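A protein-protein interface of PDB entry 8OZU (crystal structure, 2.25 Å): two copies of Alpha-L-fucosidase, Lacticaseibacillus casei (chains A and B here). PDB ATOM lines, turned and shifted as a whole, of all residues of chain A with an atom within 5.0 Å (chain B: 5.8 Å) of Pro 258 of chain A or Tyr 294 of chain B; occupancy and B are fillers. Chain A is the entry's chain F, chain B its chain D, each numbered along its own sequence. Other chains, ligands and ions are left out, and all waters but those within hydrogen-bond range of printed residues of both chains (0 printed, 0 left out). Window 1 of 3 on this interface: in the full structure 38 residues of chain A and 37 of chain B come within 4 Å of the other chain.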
ATOM      1  N   LYS A 256      30.820  21.237  11.083  1.00  0.00           N
ATOM      2  CA  LYS A 256      30.603  20.057  10.262  1.00  0.00           C
ATOM      3  C   LYS A 256      29.107  19.790  10.162  1.00  0.00           C
ATOM      4  O   LYS A 256      28.297  20.280  10.949  1.00  0.00           O
ATOM      5  CB  LYS A 256      31.329  18.886  10.912  1.00  0.00           C
ATOM      6  CG  LYS A 256      32.848  19.088  10.964  1.00  0.00           C
ATOM      7  CD  LYS A 256      33.552  17.982  11.707  1.00  0.00           C
ATOM      8  CE  LYS A 256      35.040  18.166  11.831  1.00  0.00           C
ATOM      9  NZ  LYS A 256      35.352  19.373  12.620  1.00  0.00           N
ATOM     10  N   SER A 257      28.742  19.025   9.164  1.00  0.00           N
ATOM     11  CA  SER A 257      27.354  18.643   9.026  1.00  0.00           C
ATOM     12  C   SER A 257      27.048  17.605  10.092  1.00  0.00           C
ATOM     13  O   SER A 257      27.887  16.797  10.470  1.00  0.00           O
ATOM     14  CB  SER A 257      27.054  18.115   7.643  1.00  0.00           C
ATOM     15  OG  SER A 257      27.554  16.823   7.571  1.00  0.00           O
ATOM     16  N   PRO A 258      25.846  17.640  10.681  1.00  0.00           N
ATOM     17  CA  PRO A 258      25.389  16.541  11.536  1.00  0.00           C
ATOM     18  C   PRO A 258      25.521  15.182  10.847  1.00  0.00           C
ATOM     19  O   PRO A 258      25.851  14.169  11.485  1.00  0.00           O
ATOM     20  CB  PRO A 258      23.921  16.937  11.764  1.00  0.00           C
ATOM     21  CG  PRO A 258      24.032  18.479  11.829  1.00  0.00           C
ATOM     22  CD  PRO A 258      24.908  18.776  10.646  1.00  0.00           C
ATOM     23  N   ALA A 259      25.332  15.183   9.524  1.00  0.00           N
ATOM     24  CA  ALA A 259      25.479  13.956   8.753  1.00  0.00           C
ATOM     25  C   ALA A 259      26.912  13.425   8.841  1.00  0.00           C
ATOM     26  O   ALA A 259      27.097  12.227   9.063  1.00  0.00           O
ATOM     27  CB  ALA A 259      25.064  14.165   7.323  1.00  0.00           C
ATOM     28  N   GLU A 260      27.919  14.297   8.702  1.00  0.00           N
ATOM     29  CA  GLU A 260      29.318  13.886   8.856  1.00  0.00           C
ATOM     30  C   GLU A 260      29.560  13.294  10.243  1.00  0.00           C
ATOM     31  O   GLU A 260      30.327  12.330  10.372  1.00  0.00           O
ATOM     32  CB  GLU A 260      30.265  15.073   8.624  1.00  0.00           C
ATOM     33  CG  GLU A 260      31.751  14.796   8.932  1.00  0.00           C
ATOM     34  CD  GLU A 260      32.721  15.851   8.385  1.00  0.00           C
ATOM     35  OE1 GLU A 260      32.246  16.873   7.825  1.00  0.00           O
ATOM     36  OE2 GLU A 260      33.950  15.738   8.617  1.00  0.00           O
ATOM     37  N   VAL A 261      28.964  13.910  11.302  1.00  0.00           N
ATOM     38  CA  VAL A 261      29.203  13.427  12.639  1.00  0.00           C
ATOM     39  C   VAL A 261      28.633  12.014  12.750  1.00  0.00           C
ATOM     40  O   VAL A 261      29.307  11.132  13.267  1.00  0.00           O
ATOM     41  CB  VAL A 261      28.593  14.368  13.694  1.00  0.00           C
ATOM     42  CG1 VAL A 261      28.609  13.799  15.116  1.00  0.00           C
ATOM     43  CG2 VAL A 261      29.272  15.738  13.656  1.00  0.00           C
ATOM     44  N   ILE A 262      27.419  11.776  12.221  1.00  0.00           N
ATOM     45  CA  ILE A 262      26.842  10.439  12.239  1.00  0.00           C
ATOM     46  C   ILE A 262      27.734   9.456  11.492  1.00  0.00           C
ATOM     47  O   ILE A 262      28.008   8.376  12.004  1.00  0.00           O
ATOM     48  CB  ILE A 262      25.400  10.433  11.706  1.00  0.00           C
ATOM     49  CG1 ILE A 262      24.480  11.165  12.693  1.00  0.00           C
ATOM     50  CG2 ILE A 262      24.936   8.990  11.504  1.00  0.00           C
ATOM     51  CD1 ILE A 262      23.123  11.557  12.113  1.00  0.00           C
ATOM     52  N   TYR A 294      23.506  19.393  17.852  1.00  0.00           N
ATOM     53  CA  TYR A 294      24.213  18.225  17.343  1.00  0.00           C
ATOM     54  C   TYR A 294      23.885  17.000  18.198  1.00  0.00           C
ATOM     55  O   TYR A 294      23.729  15.881  17.701  1.00  0.00           O
ATOM     56  CB  TYR A 294      25.727  18.455  17.296  1.00  0.00           C
ATOM     57  CG  TYR A 294      26.139  19.300  16.124  1.00  0.00           C
ATOM     58  CD1 TYR A 294      25.939  20.667  16.125  1.00  0.00           C
ATOM     59  CD2 TYR A 294      26.631  18.702  14.960  1.00  0.00           C
ATOM     60  CE1 TYR A 294      26.258  21.431  15.009  1.00  0.00           C
ATOM     61  CE2 TYR A 294      26.951  19.452  13.842  1.00  0.00           C
ATOM     62  CZ  TYR A 294      26.763  20.829  13.865  1.00  0.00           C
ATOM     63  OH  TYR A 294      27.045  21.558  12.722  1.00  0.00           O
ATOM     64  N   LEU A 297      20.427  15.600  17.286  1.00  0.00           N
ATOM     65  CA  LEU A 297      20.409  14.878  16.025  1.00  0.00           C
ATOM     66  C   LEU A 297      21.119  13.528  16.165  1.00  0.00           C
ATOM     67  O   LEU A 297      20.578  12.476  15.766  1.00  0.00           O
ATOM     68  CB  LEU A 297      21.025  15.763  14.947  1.00  0.00           C
ATOM     69  CG  LEU A 297      20.154  16.975  14.599  1.00  0.00           C
ATOM     70  CD1 LEU A 297      20.872  17.967  13.695  1.00  0.00           C
ATOM     71  CD2 LEU A 297      18.836  16.575  13.952  1.00  0.00           C
ATOM     72  N   VAL B  69      19.297  37.154  11.525  1.00  0.00           N
ATOM     73  CA  VAL B  69      20.128  36.380  10.593  1.00  0.00           C
ATOM     74  C   VAL B  69      20.607  37.279   9.440  1.00  0.00           C
ATOM     75  O   VAL B  69      21.385  36.813   8.601  1.00  0.00           O
ATOM     76  CB  VAL B  69      19.359  35.141  10.089  1.00  0.00           C
ATOM     77  CG1 VAL B  69      18.325  35.513   9.045  1.00  0.00           C
ATOM     78  CG2 VAL B  69      20.290  34.090   9.561  1.00  0.00           C
ATOM     79  N   LEU B 242      17.685  23.124   5.172  1.00  0.00           N
ATOM     80  CA  LEU B 242      18.767  22.748   6.043  1.00  0.00           C
ATOM     81  C   LEU B 242      18.908  21.241   6.049  1.00  0.00           C
ATOM     82  O   LEU B 242      20.043  20.781   6.193  1.00  0.00           O
ATOM     83  CB  LEU B 242      18.467  23.277   7.449  1.00  0.00           C
ATOM     84  CG  LEU B 242      18.385  24.797   7.587  1.00  0.00           C
ATOM     85  CD1 LEU B 242      18.096  25.183   9.041  1.00  0.00           C
ATOM     86  CD2 LEU B 242      19.667  25.451   7.138  1.00  0.00           C
ATOM     87  N   LEU B 253      17.815  13.390   9.682  1.00  0.00           N
ATOM     88  CA  LEU B 253      19.007  13.857  10.394  1.00  0.00           C
ATOM     89  C   LEU B 253      20.040  14.378   9.412  1.00  0.00           C
ATOM     90  O   LEU B 253      21.124  14.780   9.852  1.00  0.00           O
ATOM     91  CB  LEU B 253      19.609  12.702  11.195  1.00  0.00           C
ATOM     92  CG  LEU B 253      18.612  11.816  11.939  1.00  0.00           C
ATOM     93  CD1 LEU B 253      19.329  10.724  12.706  1.00  0.00           C
ATOM     94  CD2 LEU B 253      17.773  12.699  12.822  1.00  0.00           C
ATOM     95  N   TYR B 255      21.198  16.874   7.899  1.00  0.00           N
ATOM     96  CA  TYR B 255      21.375  18.313   7.879  1.00  0.00           C
ATOM     97  C   TYR B 255      22.698  18.681   7.221  1.00  0.00           C
ATOM     98  O   TYR B 255      23.689  17.947   7.325  1.00  0.00           O
ATOM     99  CB  TYR B 255      21.334  18.900   9.298  1.00  0.00           C
ATOM    100  CG  TYR B 255      19.959  19.186   9.851  1.00  0.00           C
ATOM    101  CD1 TYR B 255      19.136  18.153  10.294  1.00  0.00           C
ATOM    102  CD2 TYR B 255      19.495  20.486   9.946  1.00  0.00           C
ATOM    103  CE1 TYR B 255      17.893  18.409  10.846  1.00  0.00           C
ATOM    104  CE2 TYR B 255      18.238  20.755  10.463  1.00  0.00           C
ATOM    105  CZ  TYR B 255      17.420  19.710  10.880  1.00  0.00           C
ATOM    106  OH  TYR B 255      16.166  19.970  11.381  1.00  0.00           O
ATOM    107  N   LYS B 256      22.680  19.819   6.541  1.00  0.00           N
ATOM    108  CA  LYS B 256      23.856  20.361   5.887  1.00  0.00           C
ATOM    109  C   LYS B 256      24.778  21.001   6.892  1.00  0.00           C
ATOM    110  O   LYS B 256      24.348  21.357   7.979  1.00  0.00           O
ATOM    111  CB  LYS B 256      23.421  21.375   4.818  1.00  0.00           C
ATOM    112  CG  LYS B 256      22.641  20.720   3.687  1.00  0.00           C
ATOM    113  CD  LYS B 256      22.090  21.700   2.708  1.00  0.00           C
ATOM    114  CE  LYS B 256      21.214  21.082   1.653  1.00  0.00           C
ATOM    115  NZ  LYS B 256      20.024  20.413   2.232  1.00  0.00           N
ATOM    116  N   SER B 257      26.046  21.151   6.500  1.00  0.00           N
ATOM    117  CA  SER B 257      26.957  21.901   7.347  1.00  0.00           C
ATOM    118  C   SER B 257      26.578  23.391   7.308  1.00  0.00           C
ATOM    119  O   SER B 257      26.196  23.903   6.271  1.00  0.00           O
ATOM    120  CB  SER B 257      28.373  21.665   6.936  1.00  0.00           C
ATOM    121  OG  SER B 257      28.641  22.492   5.845  1.00  0.00           O
ATOM    122  N   PRO B 258      26.660  24.087   8.444  1.00  0.00           N
ATOM    123  CA  PRO B 258      26.558  25.558   8.444  1.00  0.00           C
ATOM    124  C   PRO B 258      27.536  26.195   7.461  1.00  0.00           C
ATOM    125  O   PRO B 258      27.234  27.206   6.836  1.00  0.00           O
ATOM    126  CB  PRO B 258      26.845  25.965   9.900  1.00  0.00           C
ATOM    127  CG  PRO B 258      26.437  24.691  10.693  1.00  0.00           C
ATOM    128  CD  PRO B 258      26.815  23.507   9.801  1.00  0.00           C
ATOM    129  N   VAL B 261      25.999  26.272   4.112  1.00  0.00           N
ATOM    130  CA  VAL B 261      24.957  27.302   4.049  1.00  0.00           C
ATOM    131  C   VAL B 261      25.595  28.665   3.788  1.00  0.00           C
ATOM    132  O   VAL B 261      25.157  29.392   2.906  1.00  0.00           O
ATOM    133  CB  VAL B 261      24.089  27.329   5.318  1.00  0.00           C
ATOM    134  CG1 VAL B 261      23.079  28.471   5.303  1.00  0.00           C
ATOM    135  CG2 VAL B 261      23.368  25.991   5.508  1.00  0.00           C
ATOM    136  N   ALA B 289      14.558  24.268  17.584  1.00  0.00           N
ATOM    137  CA  ALA B 289      15.873  24.598  18.107  1.00  0.00           C
ATOM    138  C   ALA B 289      16.973  24.403  17.038  1.00  0.00           C
ATOM    139  O   ALA B 289      17.864  25.255  16.894  1.00  0.00           O
ATOM    140  CB  ALA B 289      16.100  23.779  19.378  1.00  0.00           C
ATOM    141  N   ALA B 290      16.881  23.348  16.213  1.00  0.00           N
ATOM    142  CA  ALA B 290      17.918  23.124  15.211  1.00  0.00           C
ATOM    143  C   ALA B 290      18.032  24.320  14.260  1.00  0.00           C
ATOM    144  O   ALA B 290      19.158  24.732  13.905  1.00  0.00           O
ATOM    145  CB  ALA B 290      17.698  21.833  14.446  1.00  0.00           C
ATOM    146  N   ALA B 291      16.884  24.894  13.861  1.00  0.00           N
ATOM    147  CA  ALA B 291      16.928  25.999  12.911  1.00  0.00           C
ATOM    148  C   ALA B 291      17.623  27.201  13.545  1.00  0.00           C
ATOM    149  O   ALA B 291      18.346  27.915  12.860  1.00  0.00           O
ATOM    150  CB  ALA B 291      15.539  26.371  12.439  1.00  0.00           C
ATOM    151  N   GLN B 292      17.380  27.425  14.849  1.00  0.00           N
ATOM    152  CA  GLN B 292      17.975  28.553  15.561  1.00  0.00           C
ATOM    153  C   GLN B 292      19.501  28.463  15.548  1.00  0.00           C
ATOM    154  O   GLN B 292      20.170  29.485  15.373  1.00  0.00           O
ATOM    155  CB  GLN B 292      17.507  28.660  17.019  1.00  0.00           C
ATOM    156  CG  GLN B 292      16.058  29.139  17.167  1.00  0.00           C
ATOM    157  CD  GLN B 292      15.799  30.595  16.818  1.00  0.00           C
ATOM    158  OE1 GLN B 292      16.665  31.369  16.372  1.00  0.00           O
ATOM    159  NE2 GLN B 292      14.579  31.001  17.080  1.00  0.00           N
ATOM    160  N   THR B 293      20.068  27.265  15.727  1.00  0.00           N
ATOM    161  CA  THR B 293      21.509  27.118  15.644  1.00  0.00           C
ATOM    162  C   THR B 293      22.069  27.626  14.301  1.00  0.00           C
ATOM    163  O   THR B 293      23.044  28.372  14.284  1.00  0.00           O
ATOM    164  CB  THR B 293      21.910  25.681  15.987  1.00  0.00           C
ATOM    165  OG1 THR B 293      21.136  24.653  15.393  1.00  0.00           O
ATOM    166  CG2 THR B 293      21.785  25.441  17.461  1.00  0.00           C
ATOM    167  N   TYR B 294      21.419  27.276  13.187  1.00  0.00           N
ATOM    168  CA  TYR B 294      21.909  27.683  11.866  1.00  0.00           C
ATOM    169  C   TYR B 294      21.755  29.189  11.705  1.00  0.00           C
ATOM    170  O   TYR B 294      22.581  29.863  11.120  1.00  0.00           O
ATOM    171  CB  TYR B 294      21.192  26.963  10.700  1.00  0.00           C
ATOM    172  CG  TYR B 294      21.669  25.559  10.538  1.00  0.00           C
ATOM    173  CD1 TYR B 294      21.299  24.567  11.439  1.00  0.00           C
ATOM    174  CD2 TYR B 294      22.581  25.238   9.559  1.00  0.00           C
ATOM    175  CE1 TYR B 294      21.786  23.273  11.337  1.00  0.00           C
ATOM    176  CE2 TYR B 294      23.062  23.950   9.454  1.00  0.00           C
ATOM    177  CZ  TYR B 294      22.696  22.962  10.349  1.00  0.00           C
ATOM    178  OH  TYR B 294      23.155  21.671  10.193  1.00  0.00           O
ATOM    179  N   MET B 295      20.663  29.718  12.229  1.00  0.00           N
ATOM    180  CA  MET B 295      20.402  31.135  12.088  1.00  0.00           C
ATOM    181  C   MET B 295      21.450  31.948  12.849  1.00  0.00           C
ATOM    182  O   MET B 295      21.812  33.026  12.373  1.00  0.00           O
ATOM    183  CB  MET B 295      19.029  31.454  12.664  1.00  0.00           C
ATOM    184  CG  MET B 295      17.957  30.639  12.038  1.00  0.00           C
ATOM    185  SD  MET B 295      17.467  31.478  10.631  1.00  0.00           S
ATOM    186  CE  MET B 295      16.031  32.132  11.447  1.00  0.00           C
ATOM    187  N   HIS B 296      21.866  31.464  14.037  1.00  0.00           N
ATOM    188  CA  HIS B 296      22.851  32.177  14.824  1.00  0.00           C
ATOM    189  C   HIS B 296      24.193  32.142  14.101  1.00  0.00           C
ATOM    190  O   HIS B 296      24.845  33.176  14.003  1.00  0.00           O
ATOM    191  CB  HIS B 296      22.892  31.699  16.291  1.00  0.00           C
ATOM    192  CG  HIS B 296      21.658  32.081  17.060  1.00  0.00           C
ATOM    193  ND1 HIS B 296      21.174  31.397  18.150  1.00  0.00           N
ATOM    194  CD2 HIS B 296      20.747  33.051  16.814  1.00  0.00           C
ATOM    195  CE1 HIS B 296      20.051  31.979  18.578  1.00  0.00           C
ATOM    196  NE2 HIS B 296      19.760  32.976  17.766  1.00  0.00           N
ATOM    197  N   LEU B 297      24.572  30.994  13.520  1.00  0.00           N
ATOM    198  CA  LEU B 297      25.861  30.904  12.851  1.00  0.00           C
ATOM    199  C   LEU B 297      25.869  31.754  11.584  1.00  0.00           C
ATOM    200  O   LEU B 297      26.796  32.532  11.355  1.00  0.00           O
ATOM    201  CB  LEU B 297      26.182  29.438  12.559  1.00  0.00           C
ATOM    202  CG  LEU B 297      26.447  28.601  13.813  1.00  0.00           C
ATOM    203  CD1 LEU B 297      26.532  27.121  13.513  1.00  0.00           C
ATOM    204  CD2 LEU B 297      27.729  29.015  14.461  1.00  0.00           C
ATOM    205  N   LEU B 298      24.816  31.631  10.785  1.00  0.00           N
ATOM    206  CA  LEU B 298      24.764  32.384   9.558  1.00  0.00           C
ATOM    207  C   LEU B 298      24.735  33.861   9.888  1.00  0.00           C
ATOM    208  O   LEU B 298      25.327  34.673   9.173  1.00  0.00           O
ATOM    209  CB  LEU B 298      23.515  31.979   8.763  1.00  0.00           C
ATOM    210  CG  LEU B 298      23.250  32.799   7.500  1.00  0.00           C
ATOM    211  CD1 LEU B 298      24.471  32.730   6.571  1.00  0.00           C
ATOM    212  CD2 LEU B 298      21.996  32.285   6.786  1.00  0.00           C
ATOM    213  N   GLY B 299      23.980  34.204  10.945  1.00  0.00           N
ATOM    214  CA  GLY B 299      23.849  35.583  11.401  1.00  0.00           C
ATOM    215  C   GLY B 299      25.208  36.237  11.715  1.00  0.00           C
ATOM    216  O   GLY B 299      25.402  37.413  11.397  1.00  0.00           O
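Of the 19 printed residues of chain B, 6 touch a printed residue of chain A. Hydrophobic or aromatic side chains of chain B within 4 Å of the printed part of chain A: Leu 253, Tyr 255, Pro 258 and Tyr 294. Along chain B the printed residues that touch a printed residue of chain A span positions 253 to 294. Printed residues of chain A that touch a printed residue of chain B: Lys 256, Ser 257, Pro 258, Ala 259, Ile 262, Tyr 294 and Leu 297. Hydrophobic or aromatic side chains of chain A within 4 Å of the printed part of chain B: Pro 258, Ile 262, Tyr 294 and Leu 297. Among the printed residues, no Asp or Glu carboxylate lies within 4 Å of a Lys or Arg side-chain nitrogen of the other chain.
Among the printed residues, pairs that only touch across the chains: Lys 256 of chain A with Ser 257 of chain B (3.8 Å), Lys 256 of chain A with Pro 258 of chain B (3.7 Å), Ser 257 of chain A with Tyr 255 of chain B (3.4 Å), Ser 257 of chain A with Lys 256 of chain B (3.8 Å), Ser 257 of chain A with Ser 257 of chain B (3.4 Å), Pro 258 of chain A with Tyr 255 of chain B (3.6 Å), Pro 258 of chain A with Lys 256 of chain B (3.8 Å), Pro 258 of chain A with Tyr 294 of chain B (3.4 Å), Ala 259 of chain A with Tyr 255 of chain B (3.9 Å), Ile 262 of chain A with Leu 253 of chain B (3.8 Å), Tyr 294 of chain A with Pro 258 of chain B (3.5 Å), Leu 297 of chain A with Leu 253 of chain B (3.7 Å) and Leu 297 of chain A with Tyr 255 of chain B (3.7 Å).
The backbone carbonyl oxygen of Leu 242 of chain B lies within hydrogen-bond range of the backbone NH of Lys 256 of chain B, at 2.8 Å. The backbone carbonyl oxygen of Lys 256 of chain B lies within hydrogen-bond range of the side-chain hydroxyl of Tyr 294 of chain B (2.5 Å). O of Lys 256 of chain A lies within hydrogen-bond range of OH of Tyr 294 of chain A (2.5 Å). The side-chain hydroxyl (OG) of Ser 257 of chain A lies close to the backbone NH (N) of Ala 259 of chain A, at 3.4 Å. N of Glu 260 of chain A is in hydrogen-bond range of OG of Ser 257 of chain A (2.8 Å).
Printed residues of chain B within 4 Å of Pro 258 of chain A: Tyr 255, Lys 256 and Tyr 294. Printed residues of chain B within 4 Å of Ile 262 of chain A: Leu 253 (3.8 Å). Of the printed residues of chain A, Leu 253 of chain B touches Ile 262 and Leu 297. Of the printed residues of chain A, Lys 256 of chain B touches Ser 257 (3.8 Å) and Pro 258 (3.8 Å). Of the printed residues of chain A, Ser 257 of chain B touches Lys 256 (3.8 Å) and Ser 257 (3.4 Å). Of the printed residues of chain A, Pro 258 of chain B touches Lys 256 and Tyr 294. Tyr 294 of chain B touches one residue of chain A. Met 295 of chain B touches none of the printed residues of chain A. His 296 of chain B touches none of the printed residues of chain A. The nearest printed residue of chain B that does not touch Pro 258 of chain A is Leu 253 of chain B (4.02 Å). The nearest printed residue of chain A that does not touch Leu 253 of chain B is Pro 258 of chain A (4.02 Å).
Lys 256 of chain A touches Ser 257 of chain B, and with the chains exchanged Ser 257 of chain A touches Lys 256 of chain B. Lys 256 of chain A touches Pro 258 of chain B, and with the chains exchanged Pro 258 of chain A touches Lys 256 of chain B. Ser 257 of chain A touches its own counterpart, Ser 257 of chain B. Pro 258 of chain A touches Tyr 294 of chain B, and with the chains exchanged Tyr 294 of chain A touches Pro 258 of chain B. Positions printed for both chains: 256, 257, 258, 261, 294 and 297.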
